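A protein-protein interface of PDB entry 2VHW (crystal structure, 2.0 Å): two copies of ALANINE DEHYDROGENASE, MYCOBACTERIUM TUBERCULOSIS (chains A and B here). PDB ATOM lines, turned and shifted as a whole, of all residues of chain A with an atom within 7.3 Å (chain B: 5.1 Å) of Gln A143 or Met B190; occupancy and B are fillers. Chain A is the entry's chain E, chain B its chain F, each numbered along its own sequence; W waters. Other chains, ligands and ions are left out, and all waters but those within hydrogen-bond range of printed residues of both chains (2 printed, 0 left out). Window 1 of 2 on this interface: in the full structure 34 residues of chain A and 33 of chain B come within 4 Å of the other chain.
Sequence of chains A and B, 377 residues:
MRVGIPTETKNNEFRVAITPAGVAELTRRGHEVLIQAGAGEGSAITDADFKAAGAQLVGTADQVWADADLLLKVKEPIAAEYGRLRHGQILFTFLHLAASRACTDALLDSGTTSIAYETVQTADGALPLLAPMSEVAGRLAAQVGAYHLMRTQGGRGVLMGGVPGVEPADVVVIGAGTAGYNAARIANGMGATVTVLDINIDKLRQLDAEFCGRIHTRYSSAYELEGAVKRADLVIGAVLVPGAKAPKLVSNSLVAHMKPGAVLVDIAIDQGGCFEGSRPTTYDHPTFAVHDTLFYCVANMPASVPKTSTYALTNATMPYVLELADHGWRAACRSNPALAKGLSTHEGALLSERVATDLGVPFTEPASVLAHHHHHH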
ATOM      1  N   VAL A 136      -5.028   3.844   3.585  1.00  0.00           N
ATOM      2  CA  VAL A 136      -3.988   2.854   3.251  1.00  0.00           C
ATOM      3  C   VAL A 136      -3.032   2.539   4.428  1.00  0.00           C
ATOM      4  O   VAL A 136      -2.804   1.374   4.743  1.00  0.00           O
ATOM      5  CB  VAL A 136      -3.170   3.298   2.030  1.00  0.00           C
ATOM      6  CG1 VAL A 136      -1.998   2.324   1.765  1.00  0.00           C
ATOM      7  CG2 VAL A 136      -4.082   3.440   0.784  1.00  0.00           C
ATOM      8  N   ALA A 137      -2.468   3.568   5.060  1.00  0.00           N
ATOM      9  CA  ALA A 137      -1.514   3.367   6.138  1.00  0.00           C
ATOM     10  C   ALA A 137      -2.135   2.633   7.324  1.00  0.00           C
ATOM     11  O   ALA A 137      -1.494   1.782   7.925  1.00  0.00           O
ATOM     12  CB  ALA A 137      -0.900   4.717   6.583  1.00  0.00           C
ATOM     13  N   GLY A 138      -3.384   2.960   7.663  1.00  0.00           N
ATOM     14  CA  GLY A 138      -4.084   2.282   8.761  1.00  0.00           C
ATOM     15  C   GLY A 138      -4.356   0.796   8.492  1.00  0.00           C
ATOM     16  O   GLY A 138      -4.116  -0.054   9.341  1.00  0.00           O
ATOM     17  N   ARG A 139      -4.852   0.489   7.304  1.00  0.00           N
ATOM     18  CA  ARG A 139      -5.061  -0.892   6.894  1.00  0.00           C
ATOM     19  C   ARG A 139      -3.764  -1.696   6.900  1.00  0.00           C
ATOM     20  O   ARG A 139      -3.745  -2.828   7.398  1.00  0.00           O
ATOM     21  CB  ARG A 139      -5.795  -0.964   5.552  1.00  0.00           C
ATOM     22  CG  ARG A 139      -7.184  -0.370   5.683  1.00  0.00           C
ATOM     23  CD  ARG A 139      -8.056  -0.513   4.448  1.00  0.00           C
ATOM     24  NE  ARG A 139      -9.305   0.164   4.722  1.00  0.00           N
ATOM     25  CZ  ARG A 139     -10.428  -0.002   4.040  1.00  0.00           C
ATOM     26  NH1 ARG A 139     -10.489  -0.850   3.023  1.00  0.00           N
ATOM     27  NH2 ARG A 139     -11.507   0.671   4.407  1.00  0.00           N
ATOM     28  N   LEU A 140      -2.709  -1.117   6.352  1.00  0.00           N
ATOM     29  CA  LEU A 140      -1.366  -1.698   6.399  1.00  0.00           C
ATOM     30  C   LEU A 140      -0.817  -1.890   7.816  1.00  0.00           C
ATOM     31  O   LEU A 140      -0.188  -2.912   8.084  1.00  0.00           O
ATOM     32  CB  LEU A 140      -0.375  -0.884   5.580  1.00  0.00           C
ATOM     33  CG  LEU A 140      -0.381  -0.989   4.055  1.00  0.00           C
ATOM     34  CD1 LEU A 140       0.590   0.026   3.553  1.00  0.00           C
ATOM     35  CD2 LEU A 140       0.012  -2.381   3.515  1.00  0.00           C
ATOM     36  N   ALA A 141      -1.071  -0.932   8.710  1.00  0.00           N
ATOM     37  CA  ALA A 141      -0.593  -1.022  10.090  1.00  0.00           C
ATOM     38  C   ALA A 141      -1.075  -2.302  10.789  1.00  0.00           C
ATOM     39  O   ALA A 141      -0.314  -2.931  11.536  1.00  0.00           O
ATOM     40  CB  ALA A 141      -0.990   0.193  10.882  1.00  0.00           C
ATOM     41  N   ALA A 142      -2.335  -2.661  10.553  1.00  0.00           N
ATOM     42  CA  ALA A 142      -2.887  -3.888  11.102  1.00  0.00           C
ATOM     43  C   ALA A 142      -2.198  -5.136  10.555  1.00  0.00           C
ATOM     44  O   ALA A 142      -1.876  -6.039  11.324  1.00  0.00           O
ATOM     45  CB  ALA A 142      -4.398  -3.960  10.860  1.00  0.00           C
ATOM     46  N   GLN A 143      -1.977  -5.199   9.244  1.00  0.00           N
ATOM     47  CA  GLN A 143      -1.321  -6.371   8.684  1.00  0.00           C
ATOM     48  C   GLN A 143       0.158  -6.480   9.010  1.00  0.00           C
ATOM     49  O   GLN A 143       0.643  -7.592   9.225  1.00  0.00           O
ATOM     50  CB  GLN A 143      -1.567  -6.534   7.187  1.00  0.00           C
ATOM     51  CG  GLN A 143      -0.847  -5.600   6.277  1.00  0.00           C
ATOM     52  CD  GLN A 143      -1.147  -5.875   4.808  1.00  0.00           C
ATOM     53  OE1 GLN A 143      -2.300  -5.856   4.360  1.00  0.00           O
ATOM     54  NE2 GLN A 143      -0.098  -6.139   4.054  1.00  0.00           N
ATOM     55  N   VAL A 144       0.880  -5.353   9.049  1.00  0.00           N
ATOM     56  CA  VAL A 144       2.299  -5.397   9.406  1.00  0.00           C
ATOM     57  C   VAL A 144       2.495  -5.694  10.904  1.00  0.00           C
ATOM     58  O   VAL A 144       3.441  -6.383  11.292  1.00  0.00           O
ATOM     59  CB  VAL A 144       3.136  -4.145   8.910  1.00  0.00           C
ATOM     60  CG1 VAL A 144       2.968  -3.923   7.404  1.00  0.00           C
ATOM     61  CG2 VAL A 144       2.790  -2.881   9.680  1.00  0.00           C
ATOM     62  N   GLY A 145       1.594  -5.188  11.741  1.00  0.00           N
ATOM     63  CA  GLY A 145       1.660  -5.469  13.174  1.00  0.00           C
ATOM     64  C   GLY A 145       1.408  -6.948  13.461  1.00  0.00           C
ATOM     65  O   GLY A 145       2.069  -7.525  14.317  1.00  0.00           O
ATOM     66  N   ALA A 146       0.443  -7.538  12.752  1.00  0.00           N
ATOM     67  CA  ALA A 146       0.140  -8.979  12.805  1.00  0.00           C
ATOM     68  C   ALA A 146       1.333  -9.814  12.389  1.00  0.00           C
ATOM     69  O   ALA A 146       1.674 -10.792  13.051  1.00  0.00           O
ATOM     70  CB  ALA A 146      -1.018  -9.300  11.909  1.00  0.00           C
ATOM     71  N   TYR A 147       1.964  -9.413  11.291  1.00  0.00           N
ATOM     72  CA  TYR A 147       3.167 -10.078  10.789  1.00  0.00           C
ATOM     73  C   TYR A 147       4.343 -10.019  11.762  1.00  0.00           C
ATOM     74  O   TYR A 147       5.033 -11.021  11.996  1.00  0.00           O
ATOM     75  CB  TYR A 147       3.594  -9.474   9.450  1.00  0.00           C
ATOM     76  CG  TYR A 147       4.482 -10.397   8.646  1.00  0.00           C
ATOM     77  CD1 TYR A 147       5.875 -10.270   8.679  1.00  0.00           C
ATOM     78  CD2 TYR A 147       3.918 -11.411   7.852  1.00  0.00           C
ATOM     79  CE1 TYR A 147       6.694 -11.136   7.941  1.00  0.00           C
ATOM     80  CE2 TYR A 147       4.715 -12.271   7.106  1.00  0.00           C
ATOM     81  CZ  TYR A 147       6.101 -12.124   7.155  1.00  0.00           C
ATOM     82  OH  TYR A 147       6.872 -12.988   6.405  1.00  0.00           O
ATOM     83  N   HIS A 148       4.577  -8.852  12.346  1.00  0.00           N
ATOM     84  CA  HIS A 148       5.682  -8.726  13.273  1.00  0.00           C
ATOM     85  C   HIS A 148       5.419  -9.323  14.661  1.00  0.00           C
ATOM     86  O   HIS A 148       6.351  -9.510  15.439  1.00  0.00           O
ATOM     87  CB  HIS A 148       6.229  -7.296  13.310  1.00  0.00           C
ATOM     88  CG  HIS A 148       6.915  -6.914  12.041  1.00  0.00           C
ATOM     89  ND1 HIS A 148       8.237  -7.215  11.795  1.00  0.00           N
ATOM     90  CD2 HIS A 148       6.446  -6.320  10.917  1.00  0.00           C
ATOM     91  CE1 HIS A 148       8.562  -6.792  10.586  1.00  0.00           C
ATOM     92  NE2 HIS A 148       7.495  -6.242  10.033  1.00  0.00           N
ATOM     93  N   LEU A 149       4.152  -9.621  14.952  1.00  0.00           N
ATOM     94  CA  LEU A 149       3.784 -10.349  16.167  1.00  0.00           C
ATOM     95  C   LEU A 149       4.180 -11.845  16.128  1.00  0.00           C
ATOM     96  O   LEU A 149       4.166 -12.517  17.155  1.00  0.00           O
ATOM     97  CB  LEU A 149       2.279 -10.197  16.459  1.00  0.00           C
ATOM     98  CG  LEU A 149       1.808  -9.005  17.308  1.00  0.00           C
ATOM     99  CD1 LEU A 149       0.287  -9.035  17.416  1.00  0.00           C
ATOM    100  CD2 LEU A 149       2.469  -8.994  18.714  1.00  0.00           C
ATOM    101  N   MET A 160      -3.132 -12.940  15.730  1.00  0.00           N
ATOM    102  CA  MET A 160      -4.069 -11.815  15.846  1.00  0.00           C
ATOM    103  C   MET A 160      -5.407 -12.211  16.448  1.00  0.00           C
ATOM    104  O   MET A 160      -5.841 -11.640  17.440  1.00  0.00           O
ATOM    105  CB  MET A 160      -4.337 -11.155  14.484  1.00  0.00           C
ATOM    106  CG  MET A 160      -3.317 -10.117  14.079  1.00  0.00           C
ATOM    107  SD  MET A 160      -3.180  -8.674  15.138  1.00  0.00           S
ATOM    108  CE  MET A 160      -4.062  -7.383  14.208  1.00  0.00           C
ATOM    109  N   ALA A 183      -7.020   1.154  10.890  1.00  0.00           N
ATOM    110  CA  ALA A 183      -6.223   0.170  11.611  1.00  0.00           C
ATOM    111  C   ALA A 183      -7.113  -0.671  12.503  1.00  0.00           C
ATOM    112  O   ALA A 183      -7.050  -1.888  12.447  1.00  0.00           O
ATOM    113  CB  ALA A 183      -5.106   0.826  12.414  1.00  0.00           C
ATOM    114  N   ARG A 185     -10.411  -1.189  12.340  1.00  0.00           N
ATOM    115  CA  ARG A 185     -11.271  -2.005  11.505  1.00  0.00           C
ATOM    116  C   ARG A 185     -10.584  -3.294  10.986  1.00  0.00           C
ATOM    117  O   ARG A 185     -11.168  -4.398  11.045  1.00  0.00           O
ATOM    118  CB  ARG A 185     -11.822  -1.131  10.349  1.00  0.00           C
ATOM    119  CG  ARG A 185     -12.476  -1.875   9.226  1.00  0.00           C
ATOM    120  CD  ARG A 185     -13.056  -0.856   8.225  1.00  0.00           C
ATOM    121  NE  ARG A 185     -13.457  -1.476   6.954  1.00  0.00           N
ATOM    122  CZ  ARG A 185     -14.091  -0.829   5.973  1.00  0.00           C
ATOM    123  NH1 ARG A 185     -14.402   0.453   6.109  1.00  0.00           N
ATOM    124  NH2 ARG A 185     -14.393  -1.461   4.844  1.00  0.00           N
ATOM    125  N   ILE A 186      -9.369  -3.166  10.469  1.00  0.00           N
ATOM    126  CA  ILE A 186      -8.685  -4.337   9.947  1.00  0.00           C
ATOM    127  C   ILE A 186      -8.220  -5.263  11.113  1.00  0.00           C
ATOM    128  O   ILE A 186      -8.408  -6.477  11.053  1.00  0.00           O
ATOM    129  CB  ILE A 186      -7.524  -3.962   9.008  1.00  0.00           C
ATOM    130  CG1 ILE A 186      -8.012  -3.073   7.841  1.00  0.00           C
ATOM    131  CG2 ILE A 186      -6.787  -5.245   8.506  1.00  0.00           C
ATOM    132  CD1 ILE A 186      -9.214  -3.628   6.999  1.00  0.00           C
ATOM    133  N   ALA A 187      -7.665  -4.688  12.170  1.00  0.00           N
ATOM    134  CA  ALA A 187      -7.265  -5.501  13.334  1.00  0.00           C
ATOM    135  C   ALA A 187      -8.468  -6.270  13.866  1.00  0.00           C
ATOM    136  O   ALA A 187      -8.381  -7.459  14.137  1.00  0.00           O
ATOM    137  CB  ALA A 187      -6.648  -4.627  14.420  1.00  0.00           C
ATOM    138  N   ASN A 188      -9.616  -5.598  13.970  1.00  0.00           N
ATOM    139  CA  ASN A 188     -10.848  -6.250  14.395  1.00  0.00           C
ATOM    140  C   ASN A 188     -11.288  -7.311  13.405  1.00  0.00           C
ATOM    141  O   ASN A 188     -11.758  -8.377  13.815  1.00  0.00           O
ATOM    142  CB  ASN A 188     -11.965  -5.228  14.626  1.00  0.00           C
ATOM    143  CG  ASN A 188     -13.221  -5.866  15.133  1.00  0.00           C
ATOM    144  OD1 ASN A 188     -13.284  -6.335  16.260  1.00  0.00           O
ATOM    145  ND2 ASN A 188     -14.213  -5.940  14.285  1.00  0.00           N
ATOM    146  N   GLY A 189     -11.123  -7.039  12.104  1.00  0.00           N
ATOM    147  CA  GLY A 189     -11.465  -8.039  11.070  1.00  0.00           C
ATOM    148  C   GLY A 189     -10.594  -9.299  11.122  1.00  0.00           C
ATOM    149  O   GLY A 189     -11.029 -10.388  10.733  1.00  0.00           O
ATOM    150  N   MET A 190      -9.375  -9.140  11.617  1.00  0.00           N
ATOM    151  CA  MET A 190      -8.463 -10.261  11.887  1.00  0.00           C
ATOM    152  C   MET A 190      -8.749 -11.008  13.200  1.00  0.00           C
ATOM    153  O   MET A 190      -8.051 -11.969  13.515  1.00  0.00           O
ATOM    154  CB  MET A 190      -7.010  -9.781  11.849  1.00  0.00           C
ATOM    155  CG  MET A 190      -6.620  -9.185  10.461  1.00  0.00           C
ATOM    156  SD  MET A 190      -4.972  -8.488  10.348  1.00  0.00           S
ATOM    157  CE  MET A 190      -3.994  -9.978  10.134  1.00  0.00           C
ATOM    158  N   LEU A 234       0.104  -5.253  20.622  1.00  0.00           N
ATOM    159  CA  LEU A 234       0.346  -4.409  19.470  1.00  0.00           C
ATOM    160  C   LEU A 234      -0.248  -3.029  19.762  1.00  0.00           C
ATOM    161  O   LEU A 234      -1.390  -2.933  20.188  1.00  0.00           O
ATOM    162  CB  LEU A 234      -0.295  -5.021  18.208  1.00  0.00           C
ATOM    163  CG  LEU A 234      -0.396  -4.176  16.927  1.00  0.00           C
ATOM    164  CD1 LEU A 234       0.986  -3.782  16.380  1.00  0.00           C
ATOM    165  CD2 LEU A 234      -1.212  -4.928  15.850  1.00  0.00           C
ATOM    166  N   ILE A 236      -0.780   0.720  17.857  1.00  0.00           N
ATOM    167  CA  ILE A 236      -0.710   1.519  16.632  1.00  0.00           C
ATOM    168  C   ILE A 236      -0.895   3.025  16.989  1.00  0.00           C
ATOM    169  O   ILE A 236      -1.960   3.445  17.463  1.00  0.00           O
ATOM    170  CB  ILE A 236      -1.715   0.991  15.562  1.00  0.00           C
ATOM    171  CG1 ILE A 236      -1.439  -0.516  15.259  1.00  0.00           C
ATOM    172  CG2 ILE A 236      -1.679   1.868  14.296  1.00  0.00           C
ATOM    173  CD1 ILE A 236      -2.618  -1.285  14.618  1.00  0.00           C
ATOM    174  N   SER A 304       4.168   0.485  -0.554  1.00  0.00           N
ATOM    175  CA  SER A 304       4.221  -0.973  -0.764  1.00  0.00           C
ATOM    176  C   SER A 304       2.992  -1.558  -1.471  1.00  0.00           C
ATOM    177  O   SER A 304       2.993  -2.715  -1.886  1.00  0.00           O
ATOM    178  CB  SER A 304       4.461  -1.706   0.563  1.00  0.00           C
ATOM    179  OG  SER A 304       3.303  -1.646   1.379  1.00  0.00           O
ATOM    180  N   VAL A 305       1.944  -0.746  -1.595  1.00  0.00           N
ATOM    181  CA  VAL A 305       0.723  -1.156  -2.269  1.00  0.00           C
ATOM    182  C   VAL A 305       0.362  -0.127  -3.347  1.00  0.00           C
ATOM    183  O   VAL A 305      -0.726   0.435  -3.319  1.00  0.00           O
ATOM    184  CB  VAL A 305      -0.438  -1.387  -1.261  1.00  0.00           C
ATOM    185  CG1 VAL A 305      -0.204  -2.673  -0.464  1.00  0.00           C
ATOM    186  CG2 VAL A 305      -0.646  -0.167  -0.323  1.00  0.00           C
ATOM    187  N   ALA B 142      -4.000 -16.065   5.537  1.00  0.00           N
ATOM    188  CA  ALA B 142      -4.541 -14.746   5.147  1.00  0.00           C
ATOM    189  C   ALA B 142      -3.566 -13.606   5.467  1.00  0.00           C
ATOM    190  O   ALA B 142      -3.326 -12.737   4.607  1.00  0.00           O
ATOM    191  CB  ALA B 142      -5.887 -14.491   5.794  1.00  0.00           C
ATOM    192  N   GLN B 143      -3.016 -13.585   6.686  1.00  0.00           N
ATOM    193  CA  GLN B 143      -2.085 -12.504   7.058  1.00  0.00           C
ATOM    194  C   GLN B 143      -0.741 -12.580   6.298  1.00  0.00           C
ATOM    195  O   GLN B 143      -0.209 -11.570   5.860  1.00  0.00           O
ATOM    196  CB  GLN B 143      -1.883 -12.424   8.587  1.00  0.00           C
ATOM    197  CG  GLN B 143      -0.850 -13.362   9.149  1.00  0.00           C
ATOM    198  CD  GLN B 143      -0.637 -13.185  10.624  1.00  0.00           C
ATOM    199  OE1 GLN B 143       0.515 -13.187  11.094  1.00  0.00           O
ATOM    200  NE2 GLN B 143      -1.719 -13.033  11.374  1.00  0.00           N
ATOM    201  N   ALA B 146      -1.445 -11.565   2.619  1.00  0.00           N
ATOM    202  CA  ALA B 146      -1.527 -10.095   2.570  1.00  0.00           C
ATOM    203  C   ALA B 146      -0.146  -9.461   2.562  1.00  0.00           C
ATOM    204  O   ALA B 146       0.102  -8.473   1.846  1.00  0.00           O
ATOM    205  CB  ALA B 146      -2.316  -9.567   3.734  1.00  0.00           C
ATOM    206  N   TYR B 147       0.755 -10.024   3.362  1.00  0.00           N
ATOM    207  CA  TYR B 147       2.106  -9.492   3.496  1.00  0.00           C
ATOM    208  C   TYR B 147       2.904  -9.635   2.209  1.00  0.00           C
ATOM    209  O   TYR B 147       3.571  -8.688   1.761  1.00  0.00           O
ATOM    210  CB  TYR B 147       2.827 -10.166   4.646  1.00  0.00           C
ATOM    211  CG  TYR B 147       4.087  -9.441   5.056  1.00  0.00           C
ATOM    212  CD1 TYR B 147       4.021  -8.297   5.866  1.00  0.00           C
ATOM    213  CD2 TYR B 147       5.343  -9.889   4.636  1.00  0.00           C
ATOM    214  CE1 TYR B 147       5.180  -7.620   6.258  1.00  0.00           C
ATOM    215  CE2 TYR B 147       6.513  -9.214   5.021  1.00  0.00           C
ATOM    216  CZ  TYR B 147       6.420  -8.093   5.830  1.00  0.00           C
ATOM    217  OH  TYR B 147       7.569  -7.425   6.216  1.00  0.00           O
ATOM    218  N   MET B 150       2.449  -7.276  -0.849  1.00  0.00           N
ATOM    219  CA  MET B 150       3.117  -5.983  -0.865  1.00  0.00           C
ATOM    220  C   MET B 150       4.215  -6.001  -1.926  1.00  0.00           C
ATOM    221  O   MET B 150       4.910  -7.014  -2.099  1.00  0.00           O
ATOM    222  CB  MET B 150       3.700  -5.657   0.509  1.00  0.00           C
ATOM    223  CG  MET B 150       2.650  -5.408   1.559  1.00  0.00           C
ATOM    224  SD  MET B 150       3.375  -5.382   3.201  1.00  0.00           S
ATOM    225  CE  MET B 150       3.463  -3.650   3.537  1.00  0.00           C
ATOM    226  N   LEU B 159      -3.390  -3.768  -1.878  1.00  0.00           N
ATOM    227  CA  LEU B 159      -3.799  -3.853  -0.472  1.00  0.00           C
ATOM    228  C   LEU B 159      -4.992  -4.810  -0.354  1.00  0.00           C
ATOM    229  O   LEU B 159      -5.896  -4.763  -1.197  1.00  0.00           O
ATOM    230  CB  LEU B 159      -4.183  -2.447   0.014  1.00  0.00           C
ATOM    231  CG  LEU B 159      -4.592  -2.235   1.470  1.00  0.00           C
ATOM    232  CD1 LEU B 159      -3.450  -2.618   2.404  1.00  0.00           C
ATOM    233  CD2 LEU B 159      -4.968  -0.756   1.680  1.00  0.00           C
ATOM    234  N   MET B 160      -5.018  -5.670   0.675  1.00  0.00           N
ATOM    235  CA  MET B 160      -6.096  -6.678   0.826  1.00  0.00           C
ATOM    236  C   MET B 160      -7.468  -6.088   0.657  1.00  0.00           C
ATOM    237  O   MET B 160      -8.248  -6.557  -0.168  1.00  0.00           O
ATOM    238  CB  MET B 160      -6.070  -7.409   2.184  1.00  0.00           C
ATOM    239  CG  MET B 160      -5.072  -8.487   2.290  1.00  0.00           C
ATOM    240  SD  MET B 160      -5.372  -9.945   1.270  1.00  0.00           S
ATOM    241  CE  MET B 160      -6.128 -11.069   2.431  1.00  0.00           C
ATOM    242  N   GLY B 161      -7.761  -5.046   1.441  1.00  0.00           N
ATOM    243  CA  GLY B 161      -9.087  -4.489   1.464  1.00  0.00           C
ATOM    244  C   GLY B 161      -9.338  -3.327   0.517  1.00  0.00           C
ATOM    245  O   GLY B 161     -10.436  -2.807   0.485  1.00  0.00           O
ATOM    246  N   ILE B 186     -10.609 -14.657   7.764  1.00  0.00           N
ATOM    247  CA  ILE B 186      -9.653 -13.590   8.046  1.00  0.00           C
ATOM    248  C   ILE B 186      -9.418 -12.704   6.822  1.00  0.00           C
ATOM    249  O   ILE B 186      -9.317 -11.492   6.965  1.00  0.00           O
ATOM    250  CB  ILE B 186      -8.289 -14.119   8.593  1.00  0.00           C
ATOM    251  CG1 ILE B 186      -8.483 -14.976   9.861  1.00  0.00           C
ATOM    252  CG2 ILE B 186      -7.283 -12.945   8.782  1.00  0.00           C
ATOM    253  CD1 ILE B 186      -9.318 -14.320  11.019  1.00  0.00           C
ATOM    254  N   ALA B 187      -9.266 -13.306   5.640  1.00  0.00           N
ATOM    255  CA  ALA B 187      -9.119 -12.532   4.413  1.00  0.00           C
ATOM    256  C   ALA B 187     -10.302 -11.589   4.195  1.00  0.00           C
ATOM    257  O   ALA B 187     -10.131 -10.437   3.806  1.00  0.00           O
ATOM    258  CB  ALA B 187      -8.930 -13.437   3.216  1.00  0.00           C
ATOM    259  N   ASN B 188     -11.503 -12.082   4.465  1.00  0.00           N
ATOM    260  CA  ASN B 188     -12.696 -11.276   4.369  1.00  0.00           C
ATOM    261  C   ASN B 188     -12.686 -10.162   5.413  1.00  0.00           C
ATOM    262  O   ASN B 188     -13.070  -9.025   5.113  1.00  0.00           O
ATOM    263  CB  ASN B 188     -13.935 -12.173   4.514  1.00  0.00           C
ATOM    264  CG  ASN B 188     -15.223 -11.396   4.429  1.00  0.00           C
ATOM    265  OD1 ASN B 188     -15.617 -10.931   3.342  1.00  0.00           O
ATOM    266  ND2 ASN B 188     -15.871 -11.200   5.581  1.00  0.00           N
ATOM    267  N   GLY B 189     -12.240 -10.472   6.638  1.00  0.00           N
ATOM    268  CA  GLY B 189     -12.101  -9.442   7.664  1.00  0.00           C
ATOM    269  C   GLY B 189     -11.085  -8.356   7.332  1.00  0.00           C
ATOM    270  O   GLY B 189     -11.152  -7.232   7.839  1.00  0.00           O
ATOM    271  N   MET B 190     -10.116  -8.690   6.490  1.00  0.00           N
ATOM    272  CA  MET B 190      -9.151  -7.693   6.041  1.00  0.00           C
ATOM    273  C   MET B 190      -9.697  -6.867   4.873  1.00  0.00           C
ATOM    274  O   MET B 190      -9.053  -5.915   4.418  1.00  0.00           O
ATOM    275  CB  MET B 190      -7.847  -8.384   5.656  1.00  0.00           C
ATOM    276  CG  MET B 190      -7.197  -9.059   6.845  1.00  0.00           C
ATOM    277  SD  MET B 190      -5.678  -9.942   6.454  1.00  0.00           S
ATOM    278  CE  MET B 190      -4.494  -8.597   6.471  1.00  0.00           C
ATOM    279  N   GLY B 191     -10.890  -7.228   4.403  1.00  0.00           N
ATOM    280  CA  GLY B 191     -11.580  -6.425   3.393  1.00  0.00           C
ATOM    281  C   GLY B 191     -11.461  -7.002   2.002  1.00  0.00           C
ATOM    282  O   GLY B 191     -12.018  -6.450   1.072  1.00  0.00           O
ATOM    283  N   ALA B 192     -10.747  -8.118   1.843  1.00  0.00           N
ATOM    284  CA  ALA B 192     -10.636  -8.754   0.502  1.00  0.00           C
ATOM    285  C   ALA B 192     -11.959  -9.356  -0.016  1.00  0.00           C
ATOM    286  O   ALA B 192     -12.873  -9.631   0.769  1.00  0.00           O
ATOM    287  CB  ALA B 192      -9.520  -9.810   0.498  1.00  0.00           C
HETATM  288  O   HOH W   1      -0.372 -12.582  14.346  1.00  0.00           O
HETATM  289  O   HOH W   2     -12.569  -0.102   0.846  1.00  0.00           O
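NH1 of Arg A139 sits at hydrogen-bond distance from O of Gly B161 (3.2 Å).
NE2 of Gln A143 sits at hydrogen-bond distance from O of Ala B146 (3.2 Å).
The side-chain amide nitrogen (NE2) of Gln A143 lies within hydrogen-bond range of the side-chain sulfur (SD) of Met B150 (3.7 Å).
O of Ala A146 lies close to OE1 of Gln B143 (3.3 Å).
Of the 15 printed residues of chain B, 9 touch a printed residue of chain A.
Along chain B the printed residues that touch a printed residue of chain A span positions 143 to 190.
Hydrophobic or aromatic side chains of chain A within 4 Å of the printed part of chain B: Leu A140, Val A144, Ala A146, Tyr A147, His A148, Ile A186, Met A190 and Val A305.
Along chain A the printed residues that touch a printed residue of chain B span positions 139 to 305.
Among the printed residues, 19 pairs touch across the chains.
Among the printed residues, no Asp or Glu carboxylate lies within 4 Å of a Lys or Arg side-chain nitrogen of the other chain.
Gln A143 touches just these residues of chain B: Ala B146, Met B150, Leu B159 and Met B190.
Printed residues of chain B within 4 Å of Tyr A147: Tyr B147 (3.4 Å).
Of the printed residues of chain B, Ile A186 touches Met B190.
Ala A187 touches none of the printed residues of chain B.
Asn A188 touches none of the printed residues of chain B.
Of the printed residues of chain A, Ala B146 touches Gln A143.
Of the printed residues of chain A, Leu B159 touches Arg A139, Leu A140, Gln A143 and Val A305.
Gly B189 touches just one residue of chain A: Gly A189 (3.3 Å).
Met B190 touches three residues of chain A.
The nearest residue of chain B that does not touch Gln A143 is Tyr B147 (4.04 Å).
N of Gly B161 lies close to O of Met B190 (3.4 Å).
Water W1 lies within hydrogen-bond range of the backbone carbonyl oxygen of Ala A146, the backbone NH of Met A160 and the side-chain amide nitrogen of Gln B143.
Water W2 lies within hydrogen-bond range of NH1 of Arg A139 and O of Gly B161.
Gln A143 touches Ala B146, and with the chains exchanged Ala A146 touches Gln B143.
Gln A143 touches Met B190, and with the chains exchanged Met A190 touches Gln B143.
Ile A186 touches Met B190, and with the chains exchanged Met A190 touches Ile B186.
Met A190 touches its own counterpart, Met B190.
Of the 19 pairs that touch across the chains among the printed residues, 9 have their exchanged pair printed and touching as well.
Among the printed residues, pairs that only touch across the chains: Ser A304 with Met B150, Gly A189 with Gly B189, Tyr A147 with Tyr B147, Ile A186 with Met B190, Met A190 with Gln B143, Leu A140 with Leu B159, Gln A143 with Met B190, Val A305 with Leu B159, Met A190 with Ile B186, Met A190 with Met B190, Leu A140 with Met B150, Val A144 with Met B150, Gln A143 with Leu B159, Arg A139 with Leu B159 and His A148 with Tyr B147.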
